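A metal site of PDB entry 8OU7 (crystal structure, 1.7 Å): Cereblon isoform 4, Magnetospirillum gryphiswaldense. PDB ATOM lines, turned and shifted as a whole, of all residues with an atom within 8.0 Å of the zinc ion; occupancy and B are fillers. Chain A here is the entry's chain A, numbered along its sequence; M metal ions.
The backbone NH of Cys 24 sits at hydrogen-bond distance from the backbone carbonyl oxygen of Gln 29, at 2.8 Å.
O of Ser 95 lies within hydrogen-bond range of N of Cys 90, 2.8 Å away.
OG of Ser 95 lies close to SG of Cys 93.
The backbone NH (N) of Gln 29 sits close to the side-chain sulfur (SG) of Cys 27 (3.6 Å).
The backbone NH (N) of Gln 26 lies close to the side-chain sulfur (SG) of Cys 24.
The side-chain sulfur of Cys 90 lies close to the backbone NH of Gln 92 (3.5 Å).
The side-chain sulfur (SG) of Cys 27 lies close to the side-chain amide nitrogen (NE2) of Gln 92, 3.2 Å away.
Four residues have an atom within 4 Å of the zinc ion: Cys 24, Cys 27, Cys 90 and Cys 93.
The zinc ion is bound by the side-chain sulfur (SG) of Cys 93 (2.3 Å).
SG of Cys 24 is bound to the zinc ion.
SG of Cys 27 is bound to the zinc ion (2.3 Å).
SG of Cys 90 is bound to the zinc ion (2.4 Å).
The zinc ion has four donor atoms within binding distance.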
ATOM      1  N   ARG A  23      12.413 -28.752 -21.145  1.00  0.00           N
ATOM      2  CA  ARG A  23      11.578 -27.694 -20.629  1.00  0.00           C
ATOM      3  C   ARG A  23      12.406 -26.435 -20.351  1.00  0.00           C
ATOM      4  O   ARG A  23      13.597 -26.500 -20.157  1.00  0.00           O
ATOM      5  CB  ARG A  23      10.943 -28.174 -19.297  1.00  0.00           C
ATOM      6  CG  ARG A  23       9.897 -29.254 -19.550  1.00  0.00           C
ATOM      7  CD  ARG A  23       9.215 -29.718 -18.250  1.00  0.00           C
ATOM      8  NE  ARG A  23       8.214 -30.745 -18.520  1.00  0.00           N
ATOM      9  CZ  ARG A  23       7.018 -30.520 -19.113  1.00  0.00           C
ATOM     10  NH1 ARG A  23       6.580 -29.299 -19.276  1.00  0.00           N
ATOM     11  NH2 ARG A  23       6.260 -31.526 -19.509  1.00  0.00           N
ATOM     12  N   CYS A  24      11.701 -25.304 -20.203  1.00  0.00           N
ATOM     13  CA  CYS A  24      12.345 -24.063 -19.816  1.00  0.00           C
ATOM     14  C   CYS A  24      12.863 -24.237 -18.380  1.00  0.00           C
ATOM     15  O   CYS A  24      12.097 -24.677 -17.512  1.00  0.00           O
ATOM     16  CB  CYS A  24      11.390 -22.878 -19.862  1.00  0.00           C
ATOM     17  SG  CYS A  24      12.099 -21.312 -19.193  1.00  0.00           S
ATOM     18  N   ARG A  25      14.128 -23.948 -18.133  1.00  0.00           N
ATOM     19  CA  ARG A  25      14.706 -24.172 -16.809  1.00  0.00           C
ATOM     20  C   ARG A  25      14.108 -23.228 -15.755  1.00  0.00           C
ATOM     21  O   ARG A  25      14.189 -23.588 -14.533  1.00  0.00           O
ATOM     22  CB  ARG A  25      16.246 -23.981 -16.919  1.00  0.00           C
ATOM     23  CG  ARG A  25      17.022 -23.955 -15.649  1.00  0.00           C
ATOM     24  CD  ARG A  25      18.451 -23.495 -15.995  1.00  0.00           C
ATOM     25  NE  ARG A  25      19.170 -23.602 -14.775  1.00  0.00           N
ATOM     26  CZ  ARG A  25      20.434 -23.390 -14.617  1.00  0.00           C
ATOM     27  NH1 ARG A  25      21.188 -23.269 -15.725  1.00  0.00           N
ATOM     28  NH2 ARG A  25      20.908 -23.378 -13.411  1.00  0.00           N
ATOM     29  N   GLN A  26      13.620 -22.076 -16.163  1.00  0.00           N
ATOM     30  CA  GLN A  26      13.067 -21.077 -15.226  1.00  0.00           C
ATOM     31  C   GLN A  26      11.651 -21.347 -14.764  1.00  0.00           C
ATOM     32  O   GLN A  26      11.319 -21.115 -13.607  1.00  0.00           O
ATOM     33  CB  GLN A  26      13.180 -19.697 -15.806  1.00  0.00           C
ATOM     34  CG  GLN A  26      14.645 -19.367 -16.145  1.00  0.00           C
ATOM     35  N   CYS A  27      10.815 -21.970 -15.577  1.00  0.00           N
ATOM     36  CA  CYS A  27       9.383 -22.073 -15.294  1.00  0.00           C
ATOM     37  C   CYS A  27       8.759 -23.413 -15.668  1.00  0.00           C
ATOM     38  O   CYS A  27       7.624 -23.742 -15.264  1.00  0.00           O
ATOM     39  CB  CYS A  27       8.627 -20.974 -15.965  1.00  0.00           C
ATOM     40  SG  CYS A  27       8.511 -21.254 -17.802  1.00  0.00           S
ATOM     41  N   GLY A  28       9.473 -24.284 -16.430  1.00  0.00           N
ATOM     42  CA  GLY A  28       8.906 -25.569 -16.786  1.00  0.00           C
ATOM     43  C   GLY A  28       8.078 -25.688 -18.051  1.00  0.00           C
ATOM     44  O   GLY A  28       7.648 -26.777 -18.406  1.00  0.00           O
ATOM     45  N   GLN A  29       7.922 -24.612 -18.801  1.00  0.00           N
ATOM     46  CA  GLN A  29       7.264 -24.660 -20.088  1.00  0.00           C
ATOM     47  C   GLN A  29       7.846 -25.756 -20.991  1.00  0.00           C
ATOM     48  O   GLN A  29       9.056 -25.896 -21.048  1.00  0.00           O
ATOM     49  CB  GLN A  29       7.413 -23.332 -20.774  1.00  0.00           C
ATOM     50  CG  GLN A  29       6.858 -23.253 -22.200  1.00  0.00           C
ATOM     51  CD  GLN A  29       5.391 -22.908 -22.239  1.00  0.00           C
ATOM     52  OE1 GLN A  29       4.578 -23.428 -21.480  1.00  0.00           O
ATOM     53  NE2 GLN A  29       5.029 -21.948 -23.084  1.00  0.00           N
ATOM     54  N   THR A  30       6.984 -26.543 -21.609  1.00  0.00           N
ATOM     55  CA  THR A  30       7.407 -27.545 -22.560  1.00  0.00           C
ATOM     56  C   THR A  30       8.001 -26.933 -23.826  1.00  0.00           C
ATOM     57  O   THR A  30       7.362 -26.054 -24.371  1.00  0.00           O
ATOM     58  CB  THR A  30       6.255 -28.456 -22.998  1.00  0.00           C
ATOM     59  OG1 THR A  30       5.395 -28.745 -21.892  1.00  0.00           O
ATOM     60  CG2 THR A  30       6.839 -29.692 -23.616  1.00  0.00           C
ATOM     61  N   ILE A  31       9.259 -27.277 -24.205  1.00  0.00           N
ATOM     62  CA  ILE A  31       9.910 -26.567 -25.324  1.00  0.00           C
ATOM     63  C   ILE A  31      10.270 -27.534 -26.469  1.00  0.00           C
ATOM     64  O   ILE A  31       9.988 -27.259 -27.608  1.00  0.00           O
ATOM     65  CB  ILE A  31      11.189 -25.805 -24.862  1.00  0.00           C
ATOM     66  CG1 ILE A  31      10.893 -24.753 -23.797  1.00  0.00           C
ATOM     67  CG2 ILE A  31      11.797 -25.056 -26.062  1.00  0.00           C
ATOM     68  CD1 ILE A  31       9.945 -23.641 -24.143  1.00  0.00           C
ATOM     69  N   GLY A  66       6.137 -23.728 -27.484  1.00  0.00           N
ATOM     70  CA  GLY A  66       6.043 -23.017 -26.215  1.00  0.00           C
ATOM     71  C   GLY A  66       6.907 -21.748 -26.159  1.00  0.00           C
ATOM     72  O   GLY A  66       7.105 -21.171 -25.089  1.00  0.00           O
ATOM     73  N   LEU A  89      11.778 -16.181 -27.137  1.00  0.00           N
ATOM     74  CA  LEU A  89      11.562 -16.211 -25.693  1.00  0.00           C
ATOM     75  C   LEU A  89      10.747 -17.446 -25.319  1.00  0.00           C
ATOM     76  O   LEU A  89       9.935 -17.956 -26.056  1.00  0.00           O
ATOM     77  CB  LEU A  89      10.811 -14.936 -25.294  1.00  0.00           C
ATOM     78  CG  LEU A  89      11.469 -13.601 -25.679  1.00  0.00           C
ATOM     79  CD1 LEU A  89      10.647 -12.449 -25.124  1.00  0.00           C
ATOM     80  CD2 LEU A  89      12.881 -13.502 -25.221  1.00  0.00           C
ATOM     81  N   CYS A  90      10.884 -17.809 -24.021  1.00  0.00           N
ATOM     82  CA  CYS A  90       9.918 -18.705 -23.412  1.00  0.00           C
ATOM     83  C   CYS A  90       8.570 -17.995 -23.499  1.00  0.00           C
ATOM     84  O   CYS A  90       8.423 -16.857 -23.000  1.00  0.00           O
ATOM     85  CB  CYS A  90      10.306 -18.986 -21.946  1.00  0.00           C
ATOM     86  SG  CYS A  90       9.112 -20.093 -21.171  1.00  0.00           S
ATOM     87  N   GLY A  91       7.566 -18.630 -24.060  1.00  0.00           N
ATOM     88  CA  GLY A  91       6.231 -18.084 -24.184  1.00  0.00           C
ATOM     89  C   GLY A  91       5.542 -17.862 -22.834  1.00  0.00           C
ATOM     90  O   GLY A  91       4.584 -17.123 -22.748  1.00  0.00           O
ATOM     91  N   GLN A  92       5.988 -18.572 -21.814  1.00  0.00           N
ATOM     92  CA  GLN A  92       5.407 -18.512 -20.475  1.00  0.00           C
ATOM     93  C   GLN A  92       6.095 -17.414 -19.687  1.00  0.00           C
ATOM     94  O   GLN A  92       5.502 -16.405 -19.306  1.00  0.00           O
ATOM     95  CB  GLN A  92       5.469 -19.894 -19.840  1.00  0.00           C
ATOM     96  CG  GLN A  92       4.829 -19.964 -18.478  1.00  0.00           C
ATOM     97  CD  GLN A  92       4.449 -21.381 -18.101  1.00  0.00           C
ATOM     98  OE1 GLN A  92       3.285 -21.793 -18.252  1.00  0.00           O
ATOM     99  NE2 GLN A  92       5.403 -22.135 -17.596  1.00  0.00           N
ATOM    100  N   CYS A  93       7.430 -17.494 -19.476  1.00  0.00           N
ATOM    101  CA  CYS A  93       8.104 -16.672 -18.523  1.00  0.00           C
ATOM    102  C   CYS A  93       8.872 -15.526 -19.175  1.00  0.00           C
ATOM    103  O   CYS A  93       9.234 -14.606 -18.488  1.00  0.00           O
ATOM    104  CB  CYS A  93       9.010 -17.393 -17.528  1.00  0.00           C
ATOM    105  SG  CYS A  93      10.555 -18.015 -18.304  1.00  0.00           S
ATOM    106  N   GLY A  94       9.025 -15.528 -20.489  1.00  0.00           N
ATOM    107  CA  GLY A  94       9.737 -14.472 -21.207  1.00  0.00           C
ATOM    108  C   GLY A  94      11.278 -14.566 -21.172  1.00  0.00           C
ATOM    109  O   GLY A  94      11.948 -13.672 -21.714  1.00  0.00           O
ATOM    110  N   SER A  95      11.838 -15.623 -20.598  1.00  0.00           N
ATOM    111  CA  SER A  95      13.291 -15.793 -20.600  1.00  0.00           C
ATOM    112  C   SER A  95      13.793 -16.058 -22.023  1.00  0.00           C
ATOM    113  O   SER A  95      13.128 -16.688 -22.830  1.00  0.00           O
ATOM    114  CB  SER A  95      13.703 -16.885 -19.687  1.00  0.00           C
ATOM    115  OG  SER A  95      13.436 -16.500 -18.355  1.00  0.00           O
ATOM    116  N   HIS A  96      14.968 -15.490 -22.340  1.00  0.00           N
ATOM    117  CA  HIS A  96      15.521 -15.694 -23.685  1.00  0.00           C
ATOM    118  C   HIS A  96      16.083 -17.113 -23.851  1.00  0.00           C
ATOM    119  O   HIS A  96      17.000 -17.506 -23.114  1.00  0.00           O
ATOM    120  CB  HIS A  96      16.659 -14.652 -23.836  1.00  0.00           C
ATOM    121  CG  HIS A  96      17.254 -14.834 -25.171  1.00  0.00           C
ATOM    122  ND1 HIS A  96      18.612 -14.670 -25.383  1.00  0.00           N
ATOM    123  CD2 HIS A  96      16.716 -15.199 -26.395  1.00  0.00           C
ATOM    124  CE1 HIS A  96      18.867 -14.814 -26.689  1.00  0.00           C
ATOM    125  NE2 HIS A  96      17.777 -15.155 -27.321  1.00  0.00           N
ATOM    126  N   LEU A  97      15.475 -17.939 -24.678  1.00  0.00           N
ATOM    127  CA  LEU A  97      15.893 -19.318 -24.836  1.00  0.00           C
ATOM    128  C   LEU A  97      16.721 -19.595 -26.079  1.00  0.00           C
ATOM    129  O   LEU A  97      17.335 -20.662 -26.174  1.00  0.00           O
ATOM    130  CB  LEU A  97      14.651 -20.244 -24.819  1.00  0.00           C
ATOM    131  CG  LEU A  97      13.872 -20.314 -23.511  1.00  0.00           C
ATOM    132  CD1 LEU A  97      12.778 -21.369 -23.587  1.00  0.00           C
ATOM    133  CD2 LEU A  97      14.781 -20.622 -22.364  1.00  0.00           C
ATOM    134  N   ARG A 117      19.831 -23.093 -20.745  1.00  0.00           N
ATOM    135  CA  ARG A 117      18.586 -22.465 -20.361  1.00  0.00           C
ATOM    136  C   ARG A 117      17.432 -23.495 -20.351  1.00  0.00           C
ATOM    137  O   ARG A 117      16.304 -23.052 -20.170  1.00  0.00           O
ATOM    138  CB  ARG A 117      18.345 -21.225 -21.207  1.00  0.00           C
ATOM    139  CG  ARG A 117      19.487 -20.230 -20.981  1.00  0.00           C
ATOM    140  CD  ARG A 117      19.198 -18.819 -21.464  1.00  0.00           C
ATOM    141  NE  ARG A 117      20.392 -17.989 -21.362  1.00  0.00           N
ATOM    142  CZ  ARG A 117      20.536 -16.795 -21.948  1.00  0.00           C
ATOM    143  NH1 ARG A 117      19.518 -16.152 -22.500  1.00  0.00           N
ATOM    144  NH2 ARG A 117      21.727 -16.230 -21.958  1.00  0.00           N
HETATM  145 ZN    ZN M   1      10.127 -20.122 -19.031  1.00  0.00          ZN
